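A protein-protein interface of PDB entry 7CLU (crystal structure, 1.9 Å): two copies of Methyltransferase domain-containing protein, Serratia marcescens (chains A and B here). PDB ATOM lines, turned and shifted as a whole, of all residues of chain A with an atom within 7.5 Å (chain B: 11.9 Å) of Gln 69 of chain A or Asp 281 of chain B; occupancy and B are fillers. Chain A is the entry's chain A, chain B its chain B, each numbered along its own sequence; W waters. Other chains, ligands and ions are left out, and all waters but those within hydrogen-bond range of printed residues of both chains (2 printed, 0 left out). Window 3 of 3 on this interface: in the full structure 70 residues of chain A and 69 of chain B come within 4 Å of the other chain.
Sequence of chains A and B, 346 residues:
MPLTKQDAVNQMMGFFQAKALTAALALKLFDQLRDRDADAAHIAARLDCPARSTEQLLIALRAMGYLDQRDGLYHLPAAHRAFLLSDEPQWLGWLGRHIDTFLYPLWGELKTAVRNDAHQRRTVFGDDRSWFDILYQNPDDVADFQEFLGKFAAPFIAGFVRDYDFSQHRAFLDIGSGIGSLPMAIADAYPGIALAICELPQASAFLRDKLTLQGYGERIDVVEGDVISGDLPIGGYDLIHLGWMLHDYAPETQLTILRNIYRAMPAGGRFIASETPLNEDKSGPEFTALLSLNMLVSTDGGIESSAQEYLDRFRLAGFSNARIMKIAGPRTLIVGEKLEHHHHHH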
ATOM      1  N   ASP A  37      12.131 -12.745   5.475  1.00  0.00           N
ATOM      2  CA  ASP A  37      11.658 -14.115   5.379  1.00  0.00           C
ATOM      3  C   ASP A  37      12.035 -14.702   4.016  1.00  0.00           C
ATOM      4  O   ASP A  37      12.274 -13.968   3.053  1.00  0.00           O
ATOM      5  CB  ASP A  37      10.147 -14.160   5.581  1.00  0.00           C
ATOM      6  CG  ASP A  37       9.732 -13.719   6.956  1.00  0.00           C
ATOM      7  OD1 ASP A  37      10.628 -13.423   7.782  1.00  0.00           O
ATOM      8  OD2 ASP A  37       8.501 -13.667   7.218  1.00  0.00           O
ATOM      9  N   ALA A  38      12.091 -16.036   3.938  1.00  0.00           N
ATOM     10  CA  ALA A  38      12.543 -16.680   2.708  1.00  0.00           C
ATOM     11  C   ALA A  38      12.116 -18.141   2.665  1.00  0.00           C
ATOM     12  O   ALA A  38      11.985 -18.798   3.698  1.00  0.00           O
ATOM     13  CB  ALA A  38      14.065 -16.589   2.557  1.00  0.00           C
ATOM     14  N   ASP A  39      11.932 -18.651   1.447  1.00  0.00           N
ATOM     15  CA  ASP A  39      11.568 -20.048   1.273  1.00  0.00           C
ATOM     16  C   ASP A  39      12.815 -20.925   1.286  1.00  0.00           C
ATOM     17  O   ASP A  39      13.950 -20.441   1.267  1.00  0.00           O
ATOM     18  CB  ASP A  39      10.769 -20.251  -0.016  1.00  0.00           C
ATOM     19  CG  ASP A  39      11.590 -20.005  -1.290  1.00  0.00           C
ATOM     20  OD1 ASP A  39      12.834 -19.891  -1.241  1.00  0.00           O
ATOM     21  OD2 ASP A  39      10.967 -19.926  -2.373  1.00  0.00           O
ATOM     22  N   GLU A  55      15.863 -27.979   3.020  1.00  0.00           N
ATOM     23  CA  GLU A  55      14.435 -27.965   3.325  1.00  0.00           C
ATOM     24  C   GLU A  55      14.111 -28.936   4.454  1.00  0.00           C
ATOM     25  O   GLU A  55      13.305 -28.624   5.337  1.00  0.00           O
ATOM     26  CB  GLU A  55      13.597 -28.291   2.073  1.00  0.00           C
ATOM     27  CG  GLU A  55      12.118 -27.996   2.327  1.00  0.00           C
ATOM     28  CD  GLU A  55      11.189 -28.224   1.128  1.00  0.00           C
ATOM     29  OE1 GLU A  55      11.597 -28.809   0.119  1.00  0.00           O
ATOM     30  OE2 GLU A  55      10.025 -27.786   1.211  1.00  0.00           O
ATOM     31  N   LEU A  58      15.019 -27.234   7.572  1.00  0.00           N
ATOM     32  CA  LEU A  58      14.095 -26.129   7.841  1.00  0.00           C
ATOM     33  C   LEU A  58      12.772 -26.632   8.396  1.00  0.00           C
ATOM     34  O   LEU A  58      12.246 -26.077   9.371  1.00  0.00           O
ATOM     35  CB  LEU A  58      13.862 -25.326   6.564  1.00  0.00           C
ATOM     36  CG  LEU A  58      15.074 -24.514   6.129  1.00  0.00           C
ATOM     37  CD1 LEU A  58      14.867 -24.079   4.694  1.00  0.00           C
ATOM     38  CD2 LEU A  58      15.260 -23.326   7.057  1.00  0.00           C
ATOM     39  N   ILE A  59      12.198 -27.658   7.750  1.00  0.00           N
ATOM     40  CA  ILE A  59      10.935 -28.231   8.203  1.00  0.00           C
ATOM     41  C   ILE A  59      11.061 -28.730   9.632  1.00  0.00           C
ATOM     42  O   ILE A  59      10.154 -28.549  10.449  1.00  0.00           O
ATOM     43  CB  ILE A  59      10.496 -29.358   7.252  1.00  0.00           C
ATOM     44  CG1 ILE A  59      10.091 -28.793   5.889  1.00  0.00           C
ATOM     45  CG2 ILE A  59       9.370 -30.185   7.857  1.00  0.00           C
ATOM     46  CD1 ILE A  59       9.779 -29.906   4.857  1.00  0.00           C
ATOM     47  N   ARG A  62      11.167 -25.779  11.920  1.00  0.00           N
ATOM     48  CA  ARG A  62       9.820 -25.226  12.050  1.00  0.00           C
ATOM     49  C   ARG A  62       8.989 -26.094  12.979  1.00  0.00           C
ATOM     50  O   ARG A  62       8.320 -25.596  13.895  1.00  0.00           O
ATOM     51  CB  ARG A  62       9.172 -25.136  10.671  1.00  0.00           C
ATOM     52  CG  ARG A  62       7.644 -25.101  10.703  1.00  0.00           C
ATOM     53  CD  ARG A  62       7.122 -23.839  11.395  1.00  0.00           C
ATOM     54  NE  ARG A  62       5.666 -23.794  11.402  1.00  0.00           N
ATOM     55  CZ  ARG A  62       4.897 -24.352  12.330  1.00  0.00           C
ATOM     56  NH1 ARG A  62       5.443 -25.005  13.337  1.00  0.00           N
ATOM     57  NH2 ARG A  62       3.572 -24.262  12.244  1.00  0.00           N
ATOM     58  N   LEU A  67      11.518 -21.855  14.152  1.00  0.00           N
ATOM     59  CA  LEU A  67      11.178 -20.970  13.055  1.00  0.00           C
ATOM     60  C   LEU A  67       9.674 -20.990  12.842  1.00  0.00           C
ATOM     61  O   LEU A  67       8.993 -21.961  13.197  1.00  0.00           O
ATOM     62  CB  LEU A  67      11.876 -21.382  11.760  1.00  0.00           C
ATOM     63  CG  LEU A  67      13.400 -21.361  11.705  1.00  0.00           C
ATOM     64  CD1 LEU A  67      13.875 -21.969  10.398  1.00  0.00           C
ATOM     65  CD2 LEU A  67      13.937 -19.911  11.884  1.00  0.00           C
ATOM     66  N   ASP A  68       9.171 -19.894  12.283  1.00  0.00           N
ATOM     67  CA  ASP A  68       7.824 -19.797  11.749  1.00  0.00           C
ATOM     68  C   ASP A  68       7.862 -20.088  10.253  1.00  0.00           C
ATOM     69  O   ASP A  68       8.887 -19.921   9.585  1.00  0.00           O
ATOM     70  CB  ASP A  68       7.233 -18.397  11.981  1.00  0.00           C
ATOM     71  CG  ASP A  68       7.026 -18.074  13.447  1.00  0.00           C
ATOM     72  OD1 ASP A  68       6.645 -18.978  14.220  1.00  0.00           O
ATOM     73  OD2 ASP A  68       7.258 -16.911  13.837  1.00  0.00           O
ATOM     74  N   GLN A  69       6.719 -20.514   9.720  1.00  0.00           N
ATOM     75  CA  GLN A  69       6.579 -20.674   8.281  1.00  0.00           C
ATOM     76  C   GLN A  69       5.176 -20.247   7.873  1.00  0.00           C
ATOM     77  O   GLN A  69       4.189 -20.777   8.383  1.00  0.00           O
ATOM     78  CB  GLN A  69       6.868 -22.116   7.857  1.00  0.00           C
ATOM     79  CG  GLN A  69       6.940 -22.357   6.353  1.00  0.00           C
ATOM     80  CD  GLN A  69       5.604 -22.810   5.774  1.00  0.00           C
ATOM     81  OE1 GLN A  69       4.859 -22.029   5.178  1.00  0.00           O
ATOM     82  NE2 GLN A  69       5.292 -24.087   5.976  1.00  0.00           N
ATOM     83  N   ARG A  70       5.084 -19.284   6.969  1.00  0.00           N
ATOM     84  CA  ARG A  70       3.789 -18.851   6.457  1.00  0.00           C
ATOM     85  C   ARG A  70       3.872 -18.844   4.944  1.00  0.00           C
ATOM     86  O   ARG A  70       4.759 -18.197   4.376  1.00  0.00           O
ATOM     87  CB  ARG A  70       3.376 -17.473   7.001  1.00  0.00           C
ATOM     88  CG  ARG A  70       4.487 -16.436   7.022  1.00  0.00           C
ATOM     89  CD  ARG A  70       3.988 -14.989   7.131  1.00  0.00           C
ATOM     90  NE  ARG A  70       5.074 -14.091   6.746  1.00  0.00           N
ATOM     91  CZ  ARG A  70       5.121 -13.400   5.608  1.00  0.00           C
ATOM     92  NH1 ARG A  70       4.118 -13.462   4.746  1.00  0.00           N
ATOM     93  NH2 ARG A  70       6.174 -12.631   5.340  1.00  0.00           N
ATOM     94  N   ASP A  71       2.976 -19.597   4.302  1.00  0.00           N
ATOM     95  CA  ASP A  71       2.878 -19.639   2.841  1.00  0.00           C
ATOM     96  C   ASP A  71       4.220 -19.982   2.205  1.00  0.00           C
ATOM     97  O   ASP A  71       4.599 -19.424   1.179  1.00  0.00           O
ATOM     98  CB  ASP A  71       2.345 -18.314   2.266  1.00  0.00           C
ATOM     99  CG  ASP A  71       1.204 -17.735   3.072  1.00  0.00           C
ATOM    100  OD1 ASP A  71       0.247 -18.477   3.397  1.00  0.00           O
ATOM    101  OD2 ASP A  71       1.265 -16.524   3.395  1.00  0.00           O
ATOM    102  N   GLY A  72       4.958 -20.901   2.826  1.00  0.00           N
ATOM    103  CA  GLY A  72       6.220 -21.347   2.275  1.00  0.00           C
ATOM    104  C   GLY A  72       7.436 -20.524   2.664  1.00  0.00           C
ATOM    105  O   GLY A  72       8.563 -20.970   2.414  1.00  0.00           O
ATOM    106  N   LEU A  73       7.252 -19.360   3.279  1.00  0.00           N
ATOM    107  CA  LEU A  73       8.360 -18.508   3.699  1.00  0.00           C
ATOM    108  C   LEU A  73       8.709 -18.791   5.150  1.00  0.00           C
ATOM    109  O   LEU A  73       7.827 -18.792   6.014  1.00  0.00           O
ATOM    110  CB  LEU A  73       8.000 -17.030   3.555  1.00  0.00           C
ATOM    111  CG  LEU A  73       7.687 -16.473   2.176  1.00  0.00           C
ATOM    112  CD1 LEU A  73       6.923 -15.144   2.311  1.00  0.00           C
ATOM    113  CD2 LEU A  73       8.967 -16.282   1.402  1.00  0.00           C
ATOM    114  N   TYR A  74       9.991 -19.013   5.417  1.00  0.00           N
ATOM    115  CA  TYR A  74      10.454 -19.220   6.779  1.00  0.00           C
ATOM    116  C   TYR A  74      10.734 -17.873   7.423  1.00  0.00           C
ATOM    117  O   TYR A  74      11.226 -16.947   6.773  1.00  0.00           O
ATOM    118  CB  TYR A  74      11.703 -20.117   6.802  1.00  0.00           C
ATOM    119  CG  TYR A  74      11.331 -21.536   6.447  1.00  0.00           C
ATOM    120  CD1 TYR A  74      10.903 -22.421   7.430  1.00  0.00           C
ATOM    121  CD2 TYR A  74      11.335 -21.970   5.127  1.00  0.00           C
ATOM    122  CE1 TYR A  74      10.508 -23.701   7.111  1.00  0.00           C
ATOM    123  CE2 TYR A  74      10.954 -23.262   4.799  1.00  0.00           C
ATOM    124  CZ  TYR A  74      10.532 -24.115   5.803  1.00  0.00           C
ATOM    125  OH  TYR A  74      10.152 -25.399   5.508  1.00  0.00           O
ATOM    126  N   HIS A  75      10.392 -17.764   8.702  1.00  0.00           N
ATOM    127  CA  HIS A  75      10.522 -16.523   9.441  1.00  0.00           C
ATOM    128  C   HIS A  75      11.222 -16.787  10.768  1.00  0.00           C
ATOM    129  O   HIS A  75      10.830 -17.690  11.515  1.00  0.00           O
ATOM    130  CB  HIS A  75       9.142 -15.879   9.669  1.00  0.00           C
ATOM    131  CG  HIS A  75       9.152 -14.795  10.696  1.00  0.00           C
ATOM    132  ND1 HIS A  75       9.695 -13.552  10.455  1.00  0.00           N
ATOM    133  CD2 HIS A  75       8.685 -14.768  11.967  1.00  0.00           C
ATOM    134  CE1 HIS A  75       9.582 -12.809  11.542  1.00  0.00           C
ATOM    135  NE2 HIS A  75       8.961 -13.518  12.470  1.00  0.00           N
ATOM    136  N   LEU A  76      12.247 -15.992  11.056  1.00  0.00           N
ATOM    137  CA  LEU A  76      12.906 -16.049  12.360  1.00  0.00           C
ATOM    138  C   LEU A  76      12.098 -15.291  13.410  1.00  0.00           C
ATOM    139  O   LEU A  76      11.939 -14.070  13.293  1.00  0.00           O
ATOM    140  CB  LEU A  76      14.308 -15.471  12.267  1.00  0.00           C
ATOM    141  CG  LEU A  76      15.086 -15.442  13.577  1.00  0.00           C
ATOM    142  CD1 LEU A  76      15.336 -16.873  14.079  1.00  0.00           C
ATOM    143  CD2 LEU A  76      16.412 -14.705  13.392  1.00  0.00           C
ATOM    144  N   PRO A  77      11.581 -15.957  14.440  1.00  0.00           N
ATOM    145  CA  PRO A  77      10.816 -15.244  15.471  1.00  0.00           C
ATOM    146  C   PRO A  77      11.676 -14.216  16.196  1.00  0.00           C
ATOM    147  O   PRO A  77      12.861 -14.443  16.457  1.00  0.00           O
ATOM    148  CB  PRO A  77      10.364 -16.366  16.416  1.00  0.00           C
ATOM    149  CG  PRO A  77      10.334 -17.597  15.535  1.00  0.00           C
ATOM    150  CD  PRO A  77      11.503 -17.420  14.600  1.00  0.00           C
ATOM    151  N   PRO B 277       3.216 -39.451   6.488  1.00  0.00           N
ATOM    152  CA  PRO B 277       3.426 -38.234   5.700  1.00  0.00           C
ATOM    153  C   PRO B 277       3.596 -37.000   6.577  1.00  0.00           C
ATOM    154  O   PRO B 277       3.079 -36.919   7.694  1.00  0.00           O
ATOM    155  CB  PRO B 277       2.149 -38.125   4.846  1.00  0.00           C
ATOM    156  CG  PRO B 277       1.409 -39.389   5.028  1.00  0.00           C
ATOM    157  CD  PRO B 277       1.857 -39.988   6.336  1.00  0.00           C
ATOM    158  N   LEU B 278       4.328 -36.028   6.045  1.00  0.00           N
ATOM    159  CA  LEU B 278       4.271 -34.686   6.607  1.00  0.00           C
ATOM    160  C   LEU B 278       2.868 -34.117   6.417  1.00  0.00           C
ATOM    161  O   LEU B 278       2.123 -34.531   5.515  1.00  0.00           O
ATOM    162  CB  LEU B 278       5.298 -33.775   5.932  1.00  0.00           C
ATOM    163  CG  LEU B 278       6.770 -34.136   6.154  1.00  0.00           C
ATOM    164  CD1 LEU B 278       7.645 -33.382   5.174  1.00  0.00           C
ATOM    165  CD2 LEU B 278       7.169 -33.824   7.590  1.00  0.00           C
ATOM    166  N   ASN B 279       2.504 -33.169   7.283  1.00  0.00           N
ATOM    167  CA  ASN B 279       1.184 -32.536   7.198  1.00  0.00           C
ATOM    168  C   ASN B 279       1.115 -31.574   6.009  1.00  0.00           C
ATOM    169  O   ASN B 279       2.083 -31.375   5.264  1.00  0.00           O
ATOM    170  CB  ASN B 279       0.838 -31.842   8.513  1.00  0.00           C
ATOM    171  CG  ASN B 279       1.766 -30.669   8.839  1.00  0.00           C
ATOM    172  OD1 ASN B 279       2.401 -30.080   7.965  1.00  0.00           O
ATOM    173  ND2 ASN B 279       1.845 -30.338  10.114  1.00  0.00           N
ATOM    174  N   GLU B 280      -0.061 -30.957   5.846  1.00  0.00           N
ATOM    175  CA  GLU B 280      -0.414 -30.276   4.601  1.00  0.00           C
ATOM    176  C   GLU B 280       0.519 -29.120   4.262  1.00  0.00           C
ATOM    177  O   GLU B 280       0.766 -28.859   3.083  1.00  0.00           O
ATOM    178  CB  GLU B 280      -1.873 -29.783   4.669  1.00  0.00           C
ATOM    179  CG  GLU B 280      -2.891 -30.870   4.383  1.00  0.00           C
ATOM    180  CD  GLU B 280      -4.312 -30.504   4.800  1.00  0.00           C
ATOM    181  OE1 GLU B 280      -4.897 -31.260   5.607  1.00  0.00           O
ATOM    182  OE2 GLU B 280      -4.857 -29.478   4.315  1.00  0.00           O
ATOM    183  N   ASP B 281       1.036 -28.394   5.251  1.00  0.00           N
ATOM    184  CA  ASP B 281       1.984 -27.334   4.938  1.00  0.00           C
ATOM    185  C   ASP B 281       3.412 -27.703   5.338  1.00  0.00           C
ATOM    186  O   ASP B 281       4.254 -26.816   5.510  1.00  0.00           O
ATOM    187  CB  ASP B 281       1.546 -26.017   5.590  1.00  0.00           C
ATOM    188  CG  ASP B 281       1.736 -26.004   7.093  1.00  0.00           C
ATOM    189  OD1 ASP B 281       1.730 -27.081   7.727  1.00  0.00           O
ATOM    190  OD2 ASP B 281       1.888 -24.897   7.659  1.00  0.00           O
ATOM    191  N   LYS B 282       3.693 -29.004   5.479  1.00  0.00           N
ATOM    192  CA  LYS B 282       5.024 -29.514   5.833  1.00  0.00           C
ATOM    193  C   LYS B 282       5.630 -28.728   6.994  1.00  0.00           C
ATOM    194  O   LYS B 282       6.771 -28.278   6.945  1.00  0.00           O
ATOM    195  CB  LYS B 282       5.952 -29.512   4.616  1.00  0.00           C
ATOM    196  CG  LYS B 282       5.543 -30.561   3.577  1.00  0.00           C
ATOM    197  CD  LYS B 282       6.030 -30.231   2.174  1.00  0.00           C
ATOM    198  CE  LYS B 282       7.413 -30.826   1.909  1.00  0.00           C
ATOM    199  NZ  LYS B 282       7.729 -30.819   0.444  1.00  0.00           N
ATOM    200  N   SER B 283       4.825 -28.530   8.032  1.00  0.00           N
ATOM    201  CA  SER B 283       5.275 -27.912   9.267  1.00  0.00           C
ATOM    202  C   SER B 283       5.404 -28.939  10.376  1.00  0.00           C
ATOM    203  O   SER B 283       5.701 -28.572  11.520  1.00  0.00           O
ATOM    204  CB  SER B 283       4.301 -26.808   9.700  1.00  0.00           C
ATOM    205  OG  SER B 283       3.031 -27.362  10.014  1.00  0.00           O
ATOM    206  N   GLY B 284       5.160 -30.214  10.060  1.00  0.00           N
ATOM    207  CA  GLY B 284       5.194 -31.290  11.011  1.00  0.00           C
ATOM    208  C   GLY B 284       4.513 -32.516  10.441  1.00  0.00           C
ATOM    209  O   GLY B 284       4.313 -32.627   9.226  1.00  0.00           O
ATOM    210  N   PRO B 285       4.152 -33.475  11.305  1.00  0.00           N
ATOM    211  CA  PRO B 285       4.393 -33.466  12.755  1.00  0.00           C
ATOM    212  C   PRO B 285       5.884 -33.571  13.119  1.00  0.00           C
ATOM    213  O   PRO B 285       6.698 -34.000  12.297  1.00  0.00           O
ATOM    214  CB  PRO B 285       3.613 -34.693  13.253  1.00  0.00           C
ATOM    215  CG  PRO B 285       3.369 -35.534  12.037  1.00  0.00           C
ATOM    216  CD  PRO B 285       3.347 -34.628  10.870  1.00  0.00           C
ATOM    217  N   GLU B 286       6.221 -33.176  14.348  1.00  0.00           N
ATOM    218  CA  GLU B 286       7.621 -32.958  14.692  1.00  0.00           C
ATOM    219  C   GLU B 286       8.450 -34.231  14.511  1.00  0.00           C
ATOM    220  O   GLU B 286       9.533 -34.191  13.925  1.00  0.00           O
ATOM    221  CB  GLU B 286       7.744 -32.410  16.119  1.00  0.00           C
ATOM    222  CG  GLU B 286       9.204 -32.190  16.537  1.00  0.00           C
ATOM    223  CD  GLU B 286       9.368 -31.682  17.965  1.00  0.00           C
ATOM    224  OE1 GLU B 286       8.376 -31.206  18.557  1.00  0.00           O
ATOM    225  OE2 GLU B 286      10.503 -31.766  18.491  1.00  0.00           O
ATOM    226  N   THR B 288       7.989 -36.799  12.575  1.00  0.00           N
ATOM    227  CA  THR B 288       8.153 -37.105  11.161  1.00  0.00           C
ATOM    228  C   THR B 288       9.114 -36.126  10.504  1.00  0.00           C
ATOM    229  O   THR B 288       9.921 -36.519   9.650  1.00  0.00           O
ATOM    230  CB  THR B 288       6.796 -37.090  10.469  1.00  0.00           C
ATOM    231  OG1 THR B 288       5.940 -38.048  11.103  1.00  0.00           O
ATOM    232  CG2 THR B 288       6.925 -37.405   8.990  1.00  0.00           C
ATOM    233  N   ALA B 289       9.053 -34.849  10.900  1.00  0.00           N
ATOM    234  CA  ALA B 289      10.026 -33.889  10.402  1.00  0.00           C
ATOM    235  C   ALA B 289      11.428 -34.316  10.791  1.00  0.00           C
ATOM    236  O   ALA B 289      12.357 -34.250   9.981  1.00  0.00           O
ATOM    237  CB  ALA B 289       9.732 -32.481  10.932  1.00  0.00           C
ATOM    238  N   GLU B 304      10.883 -37.529   3.940  1.00  0.00           N
ATOM    239  CA  GLU B 304       9.444 -37.625   4.122  1.00  0.00           C
ATOM    240  C   GLU B 304       8.733 -36.670   3.165  1.00  0.00           C
ATOM    241  O   GLU B 304       9.327 -35.731   2.625  1.00  0.00           O
ATOM    242  CB  GLU B 304       9.068 -37.326   5.578  1.00  0.00           C
ATOM    243  CG  GLU B 304       9.893 -38.105   6.587  1.00  0.00           C
ATOM    244  CD  GLU B 304       9.637 -39.603   6.498  1.00  0.00           C
ATOM    245  OE1 GLU B 304       8.550 -39.991   6.017  1.00  0.00           O
ATOM    246  OE2 GLU B 304      10.524 -40.387   6.892  1.00  0.00           O
ATOM    247  N   SER B 305       7.448 -36.921   2.958  1.00  0.00           N
ATOM    248  CA  SER B 305       6.692 -36.184   1.957  1.00  0.00           C
ATOM    249  C   SER B 305       5.297 -35.873   2.486  1.00  0.00           C
ATOM    250  O   SER B 305       4.796 -36.517   3.409  1.00  0.00           O
ATOM    251  CB  SER B 305       6.604 -36.992   0.647  1.00  0.00           C
ATOM    252  OG  SER B 305       7.905 -37.214   0.127  1.00  0.00           O
ATOM    253  N   SER B 306       4.657 -34.883   1.877  1.00  0.00           N
ATOM    254  CA  SER B 306       3.259 -34.652   2.200  1.00  0.00           C
ATOM    255  C   SER B 306       2.374 -35.706   1.537  1.00  0.00           C
ATOM    256  O   SER B 306       2.795 -36.426   0.625  1.00  0.00           O
ATOM    257  CB  SER B 306       2.826 -33.254   1.753  1.00  0.00           C
ATOM    258  OG  SER B 306       2.758 -33.205   0.346  1.00  0.00           O
ATOM    259  N   ALA B 307       1.138 -35.799   2.036  1.00  0.00           N
ATOM    260  CA  ALA B 307       0.113 -36.628   1.401  1.00  0.00           C
ATOM    261  C   ALA B 307      -0.053 -36.274  -0.073  1.00  0.00           C
ATOM    262  O   ALA B 307      -0.083 -37.152  -0.941  1.00  0.00           O
ATOM    263  CB  ALA B 307      -1.216 -36.458   2.143  1.00  0.00           C
ATOM    264  N   GLN B 308      -0.166 -34.980  -0.371  1.00  0.00           N
ATOM    265  CA  GLN B 308      -0.333 -34.550  -1.757  1.00  0.00           C
ATOM    266  C   GLN B 308       0.849 -34.964  -2.620  1.00  0.00           C
ATOM    267  O   GLN B 308       0.667 -35.278  -3.799  1.00  0.00           O
ATOM    268  CB  GLN B 308      -0.523 -33.034  -1.827  1.00  0.00           C
ATOM    269  CG  GLN B 308      -1.852 -32.553  -1.268  1.00  0.00           C
ATOM    270  CD  GLN B 308      -3.017 -33.302  -1.850  1.00  0.00           C
ATOM    271  OE1 GLN B 308      -3.160 -33.394  -3.077  1.00  0.00           O
ATOM    272  NE2 GLN B 308      -3.867 -33.850  -0.977  1.00  0.00           N
ATOM    273  N   GLU B 309       2.056 -34.981  -2.059  1.00  0.00           N
ATOM    274  CA  GLU B 309       3.226 -35.379  -2.840  1.00  0.00           C
ATOM    275  C   GLU B 309       3.201 -36.876  -3.159  1.00  0.00           C
ATOM    276  O   GLU B 309       3.534 -37.284  -4.282  1.00  0.00           O
ATOM    277  CB  GLU B 309       4.504 -34.984  -2.096  1.00  0.00           C
ATOM    278  CG  GLU B 309       4.783 -33.487  -2.143  1.00  0.00           C
ATOM    279  CD  GLU B 309       5.933 -33.082  -1.244  1.00  0.00           C
ATOM    280  OE1 GLU B 309       6.214 -33.808  -0.269  1.00  0.00           O
ATOM    281  OE2 GLU B 309       6.556 -32.036  -1.505  1.00  0.00           O
ATOM    282  N   LYS B 326      -7.113 -42.840   5.978  1.00  0.00           N
ATOM    283  CA  LYS B 326      -6.565 -42.522   7.300  1.00  0.00           C
ATOM    284  C   LYS B 326      -7.057 -43.582   8.276  1.00  0.00           C
ATOM    285  O   LYS B 326      -8.211 -43.559   8.703  1.00  0.00           O
ATOM    286  CB  LYS B 326      -6.974 -41.120   7.732  1.00  0.00           C
ATOM    287  CG  LYS B 326      -6.625 -40.057   6.704  1.00  0.00           C
ATOM    288  CD  LYS B 326      -7.356 -38.749   6.986  1.00  0.00           C
ATOM    289  CE  LYS B 326      -6.983 -37.685   5.962  1.00  0.00           C
ATOM    290  NZ  LYS B 326      -7.411 -36.327   6.409  1.00  0.00           N
HETATM  291  O   HOH W   1       3.765 -23.260   9.116  1.00  0.00           O
HETATM  292  O   HOH W   2       7.810 -25.780   7.426  1.00  0.00           O
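OE2 of Glu 55 of chain A lies within salt-bridge range of NZ of Lys 282 of chain B. The side-chain amide nitrogen (NE2) of Gln 69 of chain A sits at hydrogen-bond distance from the backbone carbonyl oxygen (O) of Asp 281 of chain B (3.0 Å).
The backbone NH of Asp 71 of chain A lies within hydrogen-bond range of the side-chain amide oxygen of Gln 69 of chain A. The side-chain amide oxygen of Asn 279 of chain B lies within hydrogen-bond range of the backbone NH of Ser 283 of chain B, at 2.9 Å. OD1 of Asn 279 of chain B is in hydrogen-bond range of N of Lys 282 of chain B (3.0 Å). OD1 of Asp 281 of chain B sits at hydrogen-bond distance from OG of Ser 283 of chain B (2.6 Å). N of Gly 72 of chain A sits at hydrogen-bond distance from OE1 of Gln 69 of chain A, at 2.6 Å. OE2 of Glu 309 of chain B is in salt-bridge range of NZ of Lys 282 of chain B (2.6 Å).
CG2 of Ile 59 of chain A touches O of Lys 282 of chain B, 3.4 Å away. CG2 of Ile 59 of chain A touches CB of Ala 289 of chain B, 3.9 Å away. Ser 283 of chain B touches Arg 62 of chain A.
Of chain B, only Asp 281 (3.0 Å) comes within 4 Å of Gln 69 of chain A. Of chain A, only Gln 69 (3.0 Å) comes within 4 Å of Asp 281 of chain B. Of chain B, only Ser 283 (3.6 Å) comes within 4 Å of Arg 62 of chain A. No residue of chain B comes within 4 Å of Leu 67 of chain A. No residue of chain B comes within 4 Å of Asp 71 of chain A. No residue of chain B comes within 4 Å of Gly 72 of chain A. No residue of chain B comes within 4 Å of Tyr 74 of chain A. Of the printed residues of chain A, Ser 283 of chain B touches Arg 62. Of the printed residues of chain B, Glu 55 of chain A touches Lys 282 (3.9 Å). Printed residues of chain B within 4 Å of Ile 59 of chain A: Lys 282 (3.4 Å) and Ala 289 (3.9 Å). Of the printed residues of chain A, Lys 282 of chain B touches Glu 55 and Ile 59. Of the printed residues of chain A, Ala 289 of chain B touches Ile 59 (3.9 Å). Glu 280 of chain B touches none of the printed residues of chain A. Pro 285 of chain B touches none of the printed residues of chain A. The nearest residue of chain B that does not touch Gln 69 of chain A is Lys 282 of chain B (4.5 Å).
Hydrophobic or aromatic side chains of chain A within 4 Å of the printed part of chain B: Ile 59. Along chain A the printed residues that touch a printed residue of chain B span positions 55 to 69. Printed residues of chain B that touch a printed residue of chain A: Asp 281, Lys 282, Ser 283 and Ala 289. Among the printed residues, Asp or Glu carboxylates within 4 Å of a Lys or Arg side-chain nitrogen of the other chain: Glu 55 of chain A with Lys 282 of chain B (3.9 Å).
No position is printed for both chains. Of the 5 pairs that touch across the chains among the printed residues, none has its exchanged pair printed and touching as well.
Water W1 lies within hydrogen-bond range of O of Gln 69 of chain A (2.6 Å), OD2 of Asp 281 of chain B (2.9 Å) and NE of Arg 62 of chain A (3.0 Å). Water W2 lies within hydrogen-bond range of the backbone carbonyl oxygen of Lys 282 of chain B, the side-chain hydroxyl of Tyr 74 of chain A and the side-chain amide nitrogen of Gln 69 of chain A.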
